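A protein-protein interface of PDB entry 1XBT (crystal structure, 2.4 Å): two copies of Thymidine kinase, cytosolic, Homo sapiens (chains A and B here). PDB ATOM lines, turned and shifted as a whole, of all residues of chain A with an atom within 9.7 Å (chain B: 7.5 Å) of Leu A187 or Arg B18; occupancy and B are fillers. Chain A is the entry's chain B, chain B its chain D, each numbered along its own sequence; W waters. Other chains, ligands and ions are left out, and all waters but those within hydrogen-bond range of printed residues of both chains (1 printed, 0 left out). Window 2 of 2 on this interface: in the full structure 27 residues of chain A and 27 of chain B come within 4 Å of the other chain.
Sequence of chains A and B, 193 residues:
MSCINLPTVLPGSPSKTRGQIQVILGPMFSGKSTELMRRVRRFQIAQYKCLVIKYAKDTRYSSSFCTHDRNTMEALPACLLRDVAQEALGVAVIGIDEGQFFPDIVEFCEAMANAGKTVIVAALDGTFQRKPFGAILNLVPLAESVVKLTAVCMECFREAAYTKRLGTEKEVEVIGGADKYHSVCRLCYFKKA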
ATOM      1  N   ARG A 130      33.812  14.881  22.501  1.00  0.00           N
ATOM      2  CA  ARG A 130      34.448  13.568  22.292  1.00  0.00           C
ATOM      3  C   ARG A 130      35.281  13.524  21.005  1.00  0.00           C
ATOM      4  O   ARG A 130      35.310  12.522  20.301  1.00  0.00           O
ATOM      5  CB  ARG A 130      33.433  12.415  22.355  1.00  0.00           C
ATOM      6  CG  ARG A 130      32.735  12.265  23.709  1.00  0.00           C
ATOM      7  CD  ARG A 130      31.864  11.011  23.855  1.00  0.00           C
ATOM      8  NE  ARG A 130      31.109  10.781  22.638  1.00  0.00           N
ATOM      9  CZ  ARG A 130      30.966   9.609  22.026  1.00  0.00           C
ATOM     10  NH1 ARG A 130      31.501   8.491  22.520  1.00  0.00           N
ATOM     11  NH2 ARG A 130      30.267   9.576  20.899  1.00  0.00           N
ATOM     12  N   CYS A 153      30.457   8.267  36.715  1.00  0.00           N
ATOM     13  CA  CYS A 153      29.394   9.052  36.083  1.00  0.00           C
ATOM     14  C   CYS A 153      28.642   9.843  37.138  1.00  0.00           C
ATOM     15  O   CYS A 153      28.069   9.265  38.056  1.00  0.00           O
ATOM     16  CB  CYS A 153      28.425   8.168  35.279  1.00  0.00           C
ATOM     17  SG  CYS A 153      27.117   9.105  34.437  1.00  0.00           S
ATOM     18  N   GLU A 155      25.974  11.386  36.832  1.00  0.00           N
ATOM     19  CA  GLU A 155      24.536  11.379  36.566  1.00  0.00           C
ATOM     20  C   GLU A 155      23.866  10.022  36.845  1.00  0.00           C
ATOM     21  O   GLU A 155      22.711   9.979  37.275  1.00  0.00           O
ATOM     22  CB  GLU A 155      24.251  11.903  35.148  1.00  0.00           C
ATOM     23  CG  GLU A 155      24.693  13.358  34.974  1.00  0.00           C
ATOM     24  CD  GLU A 155      24.587  13.909  33.551  1.00  0.00           C
ATOM     25  OE1 GLU A 155      25.186  14.988  33.291  1.00  0.00           O
ATOM     26  OE2 GLU A 155      23.906  13.303  32.695  1.00  0.00           O
ATOM     27  N   CYS A 156      24.585   8.924  36.620  1.00  0.00           N
ATOM     28  CA  CYS A 156      24.046   7.595  36.906  1.00  0.00           C
ATOM     29  C   CYS A 156      24.952   6.736  37.800  1.00  0.00           C
ATOM     30  O   CYS A 156      24.554   5.650  38.227  1.00  0.00           O
ATOM     31  CB  CYS A 156      23.677   6.853  35.616  1.00  0.00           C
ATOM     32  SG  CYS A 156      25.036   5.954  34.825  1.00  0.00           S
ATOM     33  N   PHE A 157      26.164   7.229  38.069  1.00  0.00           N
ATOM     34  CA  PHE A 157      27.102   6.615  39.027  1.00  0.00           C
ATOM     35  C   PHE A 157      27.741   5.297  38.574  1.00  0.00           C
ATOM     36  O   PHE A 157      28.317   4.571  39.378  1.00  0.00           O
ATOM     37  CB  PHE A 157      26.464   6.499  40.432  1.00  0.00           C
ATOM     38  CG  PHE A 157      25.737   7.745  40.865  1.00  0.00           C
ATOM     39  CD1 PHE A 157      24.349   7.737  41.023  1.00  0.00           C
ATOM     40  CD2 PHE A 157      26.436   8.940  41.080  1.00  0.00           C
ATOM     41  CE1 PHE A 157      23.667   8.897  41.408  1.00  0.00           C
ATOM     42  CE2 PHE A 157      25.767  10.105  41.462  1.00  0.00           C
ATOM     43  CZ  PHE A 157      24.374  10.084  41.632  1.00  0.00           C
ATOM     44  N   ARG A 158      27.638   4.998  37.283  1.00  0.00           N
ATOM     45  CA  ARG A 158      28.406   3.909  36.683  1.00  0.00           C
ATOM     46  C   ARG A 158      29.779   4.449  36.230  1.00  0.00           C
ATOM     47  O   ARG A 158      30.097   5.609  36.481  1.00  0.00           O
ATOM     48  CB  ARG A 158      27.625   3.291  35.520  1.00  0.00           C
ATOM     49  CG  ARG A 158      26.635   2.245  35.971  1.00  0.00           C
ATOM     50  CD  ARG A 158      25.438   2.068  35.059  1.00  0.00           C
ATOM     51  NE  ARG A 158      24.548   1.020  35.555  1.00  0.00           N
ATOM     52  CZ  ARG A 158      24.636  -0.271  35.229  1.00  0.00           C
ATOM     53  NH1 ARG A 158      25.576  -0.699  34.385  1.00  0.00           N
ATOM     54  NH2 ARG A 158      23.776  -1.143  35.747  1.00  0.00           N
ATOM     55  N   GLU A 159      30.592   3.615  35.589  1.00  0.00           N
ATOM     56  CA  GLU A 159      31.894   4.045  35.080  1.00  0.00           C
ATOM     57  C   GLU A 159      31.749   5.107  33.979  1.00  0.00           C
ATOM     58  O   GLU A 159      30.947   4.948  33.061  1.00  0.00           O
ATOM     59  CB  GLU A 159      32.670   2.843  34.545  1.00  0.00           C
ATOM     60  CG  GLU A 159      33.981   2.576  35.268  1.00  0.00           C
ATOM     61  CD  GLU A 159      34.656   1.280  34.824  1.00  0.00           C
ATOM     62  OE1 GLU A 159      34.748   1.027  33.595  1.00  0.00           O
ATOM     63  OE2 GLU A 159      35.100   0.512  35.711  1.00  0.00           O
ATOM     64  N   ALA A 160      32.527   6.181  34.085  1.00  0.00           N
ATOM     65  CA  ALA A 160      32.507   7.261  33.106  1.00  0.00           C
ATOM     66  C   ALA A 160      33.797   7.325  32.292  1.00  0.00           C
ATOM     67  O   ALA A 160      34.901   7.255  32.844  1.00  0.00           O
ATOM     68  CB  ALA A 160      32.258   8.593  33.790  1.00  0.00           C
ATOM     69  N   ALA A 161      33.648   7.474  30.978  1.00  0.00           N
ATOM     70  CA  ALA A 161      34.800   7.591  30.080  1.00  0.00           C
ATOM     71  C   ALA A 161      34.890   8.964  29.410  1.00  0.00           C
ATOM     72  O   ALA A 161      35.908   9.288  28.799  1.00  0.00           O
ATOM     73  CB  ALA A 161      34.786   6.476  29.026  1.00  0.00           C
ATOM     74  N   TYR A 162      33.830   9.766  29.542  1.00  0.00           N
ATOM     75  CA  TYR A 162      33.711  11.033  28.819  1.00  0.00           C
ATOM     76  C   TYR A 162      33.439  12.234  29.714  1.00  0.00           C
ATOM     77  O   TYR A 162      33.079  12.088  30.883  1.00  0.00           O
ATOM     78  CB  TYR A 162      32.635  10.911  27.721  1.00  0.00           C
ATOM     79  CG  TYR A 162      32.656   9.548  27.059  1.00  0.00           C
ATOM     80  CD1 TYR A 162      31.642   8.623  27.301  1.00  0.00           C
ATOM     81  CD2 TYR A 162      33.718   9.170  26.226  1.00  0.00           C
ATOM     82  CE1 TYR A 162      31.667   7.368  26.718  1.00  0.00           C
ATOM     83  CE2 TYR A 162      33.762   7.916  25.644  1.00  0.00           C
ATOM     84  CZ  TYR A 162      32.734   7.019  25.892  1.00  0.00           C
ATOM     85  OH  TYR A 162      32.757   5.769  25.330  1.00  0.00           O
ATOM     86  N   LYS A 164      31.157  15.758  29.793  1.00  0.00           N
ATOM     87  CA  LYS A 164      30.064  16.556  29.256  1.00  0.00           C
ATOM     88  C   LYS A 164      30.172  18.001  29.753  1.00  0.00           C
ATOM     89  O   LYS A 164      30.388  18.239  30.937  1.00  0.00           O
ATOM     90  CB  LYS A 164      28.726  15.941  29.687  1.00  0.00           C
ATOM     91  CG  LYS A 164      27.485  16.653  29.208  1.00  0.00           C
ATOM     92  CD  LYS A 164      26.327  15.669  29.111  1.00  0.00           C
ATOM     93  CE  LYS A 164      25.191  16.038  30.047  1.00  0.00           C
ATOM     94  NZ  LYS A 164      24.252  14.889  30.245  1.00  0.00           N
ATOM     95  N   SER A 183      31.748  14.299  34.513  1.00  0.00           N
ATOM     96  CA  SER A 183      32.210  13.030  33.966  1.00  0.00           C
ATOM     97  C   SER A 183      30.975  12.170  33.759  1.00  0.00           C
ATOM     98  O   SER A 183      30.110  12.100  34.628  1.00  0.00           O
ATOM     99  CB  SER A 183      33.217  12.333  34.891  1.00  0.00           C
ATOM    100  OG  SER A 183      32.711  12.201  36.213  1.00  0.00           O
ATOM    101  N   VAL A 184      30.878  11.541  32.588  1.00  0.00           N
ATOM    102  CA  VAL A 184      29.661  10.814  32.192  1.00  0.00           C
ATOM    103  C   VAL A 184      29.935   9.511  31.430  1.00  0.00           C
ATOM    104  O   VAL A 184      30.945   9.374  30.747  1.00  0.00           O
ATOM    105  CB  VAL A 184      28.678  11.671  31.312  1.00  0.00           C
ATOM    106  CG1 VAL A 184      28.003  12.773  32.126  1.00  0.00           C
ATOM    107  CG2 VAL A 184      29.370  12.228  30.054  1.00  0.00           C
ATOM    108  N   CYS A 185      29.011   8.563  31.540  1.00  0.00           N
ATOM    109  CA  CYS A 185      29.033   7.371  30.691  1.00  0.00           C
ATOM    110  C   CYS A 185      28.457   7.689  29.300  1.00  0.00           C
ATOM    111  O   CYS A 185      28.000   8.803  29.050  1.00  0.00           O
ATOM    112  CB  CYS A 185      28.278   6.197  31.341  1.00  0.00           C
ATOM    113  SG  CYS A 185      26.472   6.417  31.455  1.00  0.00           S
ATOM    114  N   ARG A 186      28.487   6.703  28.409  1.00  0.00           N
ATOM    115  CA  ARG A 186      27.958   6.846  27.054  1.00  0.00           C
ATOM    116  C   ARG A 186      26.486   7.265  27.027  1.00  0.00           C
ATOM    117  O   ARG A 186      26.111   8.197  26.316  1.00  0.00           O
ATOM    118  CB  ARG A 186      28.156   5.547  26.261  1.00  0.00           C
ATOM    119  CG  ARG A 186      27.606   5.568  24.825  1.00  0.00           C
ATOM    120  CD  ARG A 186      27.881   4.292  24.023  1.00  0.00           C
ATOM    121  NE  ARG A 186      29.318   4.058  23.874  1.00  0.00           N
ATOM    122  CZ  ARG A 186      30.043   4.521  22.868  1.00  0.00           C
ATOM    123  NH1 ARG A 186      29.452   5.216  21.907  1.00  0.00           N
ATOM    124  NH2 ARG A 186      31.351   4.273  22.804  1.00  0.00           N
ATOM    125  N   LEU A 187      25.659   6.575  27.803  1.00  0.00           N
ATOM    126  CA  LEU A 187      24.217   6.843  27.827  1.00  0.00           C
ATOM    127  C   LEU A 187      23.887   8.236  28.363  1.00  0.00           C
ATOM    128  O   LEU A 187      23.079   8.950  27.767  1.00  0.00           O
ATOM    129  CB  LEU A 187      23.448   5.753  28.596  1.00  0.00           C
ATOM    130  CG  LEU A 187      23.344   4.392  27.884  1.00  0.00           C
ATOM    131  CD1 LEU A 187      22.645   3.353  28.752  1.00  0.00           C
ATOM    132  CD2 LEU A 187      22.665   4.500  26.511  1.00  0.00           C
ATOM    133  N   CYS A 188      24.526   8.624  29.468  1.00  0.00           N
ATOM    134  CA  CYS A 188      24.291   9.933  30.068  1.00  0.00           C
ATOM    135  C   CYS A 188      24.830  11.067  29.187  1.00  0.00           C
ATOM    136  O   CYS A 188      24.258  12.162  29.177  1.00  0.00           O
ATOM    137  CB  CYS A 188      24.842  10.003  31.507  1.00  0.00           C
ATOM    138  SG  CYS A 188      24.139   8.785  32.689  1.00  0.00           S
ATOM    139  N   TYR A 189      25.902  10.796  28.435  1.00  0.00           N
ATOM    140  CA  TYR A 189      26.460  11.774  27.504  1.00  0.00           C
ATOM    141  C   TYR A 189      25.436  12.221  26.447  1.00  0.00           C
ATOM    142  O   TYR A 189      25.399  13.392  26.080  1.00  0.00           O
ATOM    143  CB  TYR A 189      27.737  11.245  26.824  1.00  0.00           C
ATOM    144  CG  TYR A 189      28.369  12.251  25.873  1.00  0.00           C
ATOM    145  CD1 TYR A 189      29.293  13.185  26.334  1.00  0.00           C
ATOM    146  CD2 TYR A 189      28.012  12.285  24.516  1.00  0.00           C
ATOM    147  CE1 TYR A 189      29.859  14.122  25.478  1.00  0.00           C
ATOM    148  CE2 TYR A 189      28.577  13.218  23.644  1.00  0.00           C
ATOM    149  CZ  TYR A 189      29.505  14.128  24.129  1.00  0.00           C
ATOM    150  OH  TYR A 189      30.071  15.063  23.282  1.00  0.00           O
ATOM    151  N   PHE A 190      24.623  11.282  25.971  1.00  0.00           N
ATOM    152  CA  PHE A 190      23.675  11.535  24.891  1.00  0.00           C
ATOM    153  C   PHE A 190      22.249  11.865  25.372  1.00  0.00           C
ATOM    154  O   PHE A 190      21.375  12.156  24.550  1.00  0.00           O
ATOM    155  CB  PHE A 190      23.639  10.336  23.927  1.00  0.00           C
ATOM    156  CG  PHE A 190      24.833  10.239  23.014  1.00  0.00           C
ATOM    157  CD1 PHE A 190      25.739   9.181  23.142  1.00  0.00           C
ATOM    158  CD2 PHE A 190      25.046  11.186  22.008  1.00  0.00           C
ATOM    159  CE1 PHE A 190      26.852   9.080  22.293  1.00  0.00           C
ATOM    160  CE2 PHE A 190      26.144  11.087  21.145  1.00  0.00           C
ATOM    161  CZ  PHE A 190      27.052  10.033  21.291  1.00  0.00           C
ATOM    162  N   LYS A 191      22.024  11.827  26.688  1.00  0.00           N
ATOM    163  CA  LYS A 191      20.688  12.061  27.264  1.00  0.00           C
ATOM    164  C   LYS A 191      20.161  13.487  27.054  1.00  0.00           C
ATOM    165  O   LYS A 191      20.872  14.466  27.288  1.00  0.00           O
ATOM    166  CB  LYS A 191      20.658  11.703  28.753  1.00  0.00           C
ATOM    167  CG  LYS A 191      19.706  10.561  29.088  1.00  0.00           C
ATOM    168  CD  LYS A 191      19.617  10.323  30.594  1.00  0.00           C
ATOM    169  CE  LYS A 191      18.312  10.864  31.182  1.00  0.00           C
ATOM    170  NZ  LYS A 191      17.448   9.755  31.696  1.00  0.00           N
ATOM    171  N   ARG B  18      23.267  -1.489  26.705  1.00  0.00           N
ATOM    172  CA  ARG B  18      24.549  -0.891  27.215  1.00  0.00           C
ATOM    173  C   ARG B  18      25.763  -1.233  26.333  1.00  0.00           C
ATOM    174  O   ARG B  18      26.503  -2.194  26.589  1.00  0.00           O
ATOM    175  CB  ARG B  18      24.799  -1.296  28.672  1.00  0.00           C
ATOM    176  CG  ARG B  18      25.806  -0.415  29.392  1.00  0.00           C
ATOM    177  CD  ARG B  18      25.589  -0.303  30.904  1.00  0.00           C
ATOM    178  NE  ARG B  18      25.950   1.032  31.373  1.00  0.00           N
ATOM    179  CZ  ARG B  18      25.074   1.987  31.684  1.00  0.00           C
ATOM    180  NH1 ARG B  18      23.765   1.755  31.605  1.00  0.00           N
ATOM    181  NH2 ARG B  18      25.511   3.180  32.080  1.00  0.00           N
ATOM    182  N   GLY B  19      25.954  -0.418  25.295  1.00  0.00           N
ATOM    183  CA  GLY B  19      27.039  -0.598  24.348  1.00  0.00           C
ATOM    184  C   GLY B  19      28.354  -0.034  24.840  1.00  0.00           C
ATOM    185  O   GLY B  19      28.396   0.677  25.846  1.00  0.00           O
ATOM    186  N   GLN B  20      29.421  -0.326  24.100  1.00  0.00           N
ATOM    187  CA  GLN B  20      30.786  -0.126  24.570  1.00  0.00           C
ATOM    188  C   GLN B  20      31.778  -0.247  23.424  1.00  0.00           C
ATOM    189  O   GLN B  20      31.597  -1.083  22.534  1.00  0.00           O
ATOM    190  CB  GLN B  20      31.108  -1.247  25.546  1.00  0.00           C
ATOM    191  CG  GLN B  20      31.724  -0.836  26.824  1.00  0.00           C
ATOM    192  CD  GLN B  20      32.457  -1.983  27.484  1.00  0.00           C
ATOM    193  OE1 GLN B  20      32.020  -3.131  27.415  1.00  0.00           O
ATOM    194  NE2 GLN B  20      33.578  -1.677  28.121  1.00  0.00           N
ATOM    195  N   ALA B  92      25.562  -9.577  19.500  1.00  0.00           N
ATOM    196  CA  ALA B  92      25.750  -8.744  20.694  1.00  0.00           C
ATOM    197  C   ALA B  92      27.185  -8.213  20.866  1.00  0.00           C
ATOM    198  O   ALA B  92      27.391  -7.125  21.420  1.00  0.00           O
ATOM    199  CB  ALA B  92      25.302  -9.489  21.947  1.00  0.00           C
ATOM    200  N   MET B 112      27.534   1.015  16.220  1.00  0.00           N
ATOM    201  CA  MET B 112      27.268  -0.268  16.868  1.00  0.00           C
ATOM    202  C   MET B 112      27.188  -0.133  18.396  1.00  0.00           C
ATOM    203  O   MET B 112      26.319  -0.740  19.025  1.00  0.00           O
ATOM    204  CB  MET B 112      28.305  -1.329  16.467  1.00  0.00           C
ATOM    205  CG  MET B 112      28.229  -1.808  15.004  1.00  0.00           C
ATOM    206  SD  MET B 112      26.602  -2.469  14.468  1.00  0.00           S
ATOM    207  CE  MET B 112      26.632  -2.034  12.693  1.00  0.00           C
ATOM    208  N   ALA B 113      28.071   0.674  18.983  1.00  0.00           N
ATOM    209  CA  ALA B 113      28.075   0.880  20.437  1.00  0.00           C
ATOM    210  C   ALA B 113      26.826   1.620  20.899  1.00  0.00           C
ATOM    211  O   ALA B 113      26.274   1.315  21.950  1.00  0.00           O
ATOM    212  CB  ALA B 113      29.341   1.610  20.889  1.00  0.00           C
ATOM    213  N   ASN B 114      26.391   2.589  20.100  1.00  0.00           N
ATOM    214  CA  ASN B 114      25.157   3.323  20.358  1.00  0.00           C
ATOM    215  C   ASN B 114      23.885   2.480  20.155  1.00  0.00           C
ATOM    216  O   ASN B 114      22.839   2.795  20.710  1.00  0.00           O
ATOM    217  CB  ASN B 114      25.127   4.607  19.523  1.00  0.00           C
ATOM    218  CG  ASN B 114      26.149   5.646  20.002  1.00  0.00           C
ATOM    219  OD1 ASN B 114      26.604   5.614  21.157  1.00  0.00           O
ATOM    220  ND2 ASN B 114      26.513   6.572  19.114  1.00  0.00           N
ATOM    221  N   ALA B 115      23.986   1.411  19.368  1.00  0.00           N
ATOM    222  CA  ALA B 115      22.891   0.448  19.227  1.00  0.00           C
ATOM    223  C   ALA B 115      22.964  -0.664  20.281  1.00  0.00           C
ATOM    224  O   ALA B 115      22.238  -1.657  20.197  1.00  0.00           O
ATOM    225  CB  ALA B 115      22.841  -0.136  17.809  1.00  0.00           C
ATOM    226  N   GLY B 116      23.850  -0.499  21.268  1.00  0.00           N
ATOM    227  CA  GLY B 116      23.929  -1.403  22.405  1.00  0.00           C
ATOM    228  C   GLY B 116      24.856  -2.597  22.277  1.00  0.00           C
ATOM    229  O   GLY B 116      24.808  -3.505  23.106  1.00  0.00           O
ATOM    230  N   LYS B 117      25.700  -2.611  21.253  1.00  0.00           N
ATOM    231  CA  LYS B 117      26.664  -3.692  21.094  1.00  0.00           C
ATOM    232  C   LYS B 117      28.007  -3.427  21.796  1.00  0.00           C
ATOM    233  O   LYS B 117      28.399  -2.280  22.003  1.00  0.00           O
ATOM    234  CB  LYS B 117      26.880  -3.982  19.605  1.00  0.00           C
ATOM    235  CG  LYS B 117      25.782  -4.822  18.966  1.00  0.00           C
ATOM    236  CD  LYS B 117      24.724  -3.970  18.280  1.00  0.00           C
ATOM    237  CE  LYS B 117      23.884  -4.794  17.309  1.00  0.00           C
ATOM    238  NZ  LYS B 117      23.192  -5.934  17.960  1.00  0.00           N
ATOM    239  N   THR B 118      28.699  -4.501  22.163  1.00  0.00           N
ATOM    240  CA  THR B 118      30.075  -4.414  22.651  1.00  0.00           C
ATOM    241  C   THR B 118      31.029  -4.594  21.479  1.00  0.00           C
ATOM    242  O   THR B 118      31.044  -5.647  20.837  1.00  0.00           O
ATOM    243  CB  THR B 118      30.347  -5.476  23.736  1.00  0.00           C
ATOM    244  OG1 THR B 118      29.669  -5.098  24.931  1.00  0.00           O
ATOM    245  CG2 THR B 118      31.812  -5.466  24.172  1.00  0.00           C
ATOM    246  N   GLU B 144      35.423   3.435  25.912  1.00  0.00           N
ATOM    247  CA  GLU B 144      35.386   3.340  27.366  1.00  0.00           C
ATOM    248  C   GLU B 144      36.606   2.613  27.945  1.00  0.00           C
ATOM    249  O   GLU B 144      36.898   2.740  29.135  1.00  0.00           O
ATOM    250  CB  GLU B 144      34.048   2.801  27.901  1.00  0.00           C
ATOM    251  CG  GLU B 144      33.172   2.042  26.917  1.00  0.00           C
ATOM    252  CD  GLU B 144      32.280   2.924  26.050  1.00  0.00           C
ATOM    253  OE1 GLU B 144      31.161   3.289  26.477  1.00  0.00           O
ATOM    254  OE2 GLU B 144      32.691   3.225  24.918  1.00  0.00           O
HETATM  255  O   HOH W   1      29.981   4.292  28.826  1.00  0.00           O
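OH of Tyr A162 lies within hydrogen-bond range of OE2 of Glu B144 (2.6 Å). The guanidinium group of Arg B18 lies close to the side-chain sulfur of Cys A185 (3.4 Å). The guanidinium group of Arg A186 sits at hydrogen-bond distance from the side-chain amide oxygen of Asn B114, at 3.0 Å. NH2 of Arg A186 is in salt-bridge range of OE2 of Glu B144 (2.7 Å). The guanidinium group (NE) of Arg B18 lies close to the guanidinium group (NH1) of Arg A158 (3.5 Å).
The backbone NH (N) of Cys A153 sits at hydrogen-bond distance from the backbone carbonyl oxygen (O) of Arg A158, at 2.7 Å. The side-chain sulfur (SG) of Cys A156 lies close to the backbone NH (N) of Arg A158 (3.7 Å). The backbone NH of Ala A161 is in hydrogen-bond range of the backbone carbonyl oxygen of Val A184. N of Val A184 lies within hydrogen-bond range of O of Tyr A162 (2.8 Å). OH of Tyr A162 sits at hydrogen-bond distance from NH2 of Arg A186 (3.3 Å). SG of Cys A185 sits close to N of Leu A187 (3.7 Å).
Cys A156 touches Arg B18 (SG to NH2, 3.9 Å). Ala A161 touches Glu B144 (CB to CA, 3.6 Å). CB of Ala B113 touches CZ of Arg A186, at 3.6 Å. Arg B18 touches Leu A187 (NH1 to CD1, 3.5 Å). Phe A190 touches Asn B114.
Of the printed residues of chain B, Cys A156 touches Arg B18. Printed residues of chain B within 4 Å of Tyr A162: Glu B144 (2.6 Å). Of the printed residues of chain B, Arg A186 touches Ala B113 (3.6 Å), Asn B114 (3.0 Å) and Glu B144 (2.7 Å). Leu A187 touches just one residue of chain B: Arg B18. Of the printed residues of chain B, Phe A190 touches Asn B114 (3.7 Å). Arg B18 touches just these residues of chain A: Cys A156 (3.9 Å), Arg A158 (3.2 Å), Cys A185 (3.4 Å) and Leu A187 (3.5 Å). No residue of chain A comes within 4 Å of Gly B19. Gly B116 touches none of the printed residues of chain A. The nearest printed residue of chain B that does not touch Arg A186 is Gly B19 (4.02 Å).
Printed residues of chain B that touch a printed residue of chain A: Arg B18, Ala B113, Asn B114 and Glu B144. Hydrophobic or aromatic side chains of chain B within 4 Å of the printed part of chain A: Ala B113. Printed residues of chain A that touch a printed residue of chain B: Cys A156, Arg A158, Ala A161, Tyr A162, Cys A185, Arg A186, Leu A187 and Phe A190. Hydrophobic or aromatic side chains of chain A within 4 Å of the printed part of chain B: Ala A161, Tyr A162, Leu A187 and Phe A190. Among the printed residues, Asp or Glu carboxylates within 4 Å of a Lys or Arg side-chain nitrogen of the other chain: Arg A186 with Glu B144 (2.7 Å).
No position is printed for both chains.
Water W1 bridges OE1 of Glu B144 and N of Arg A186.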
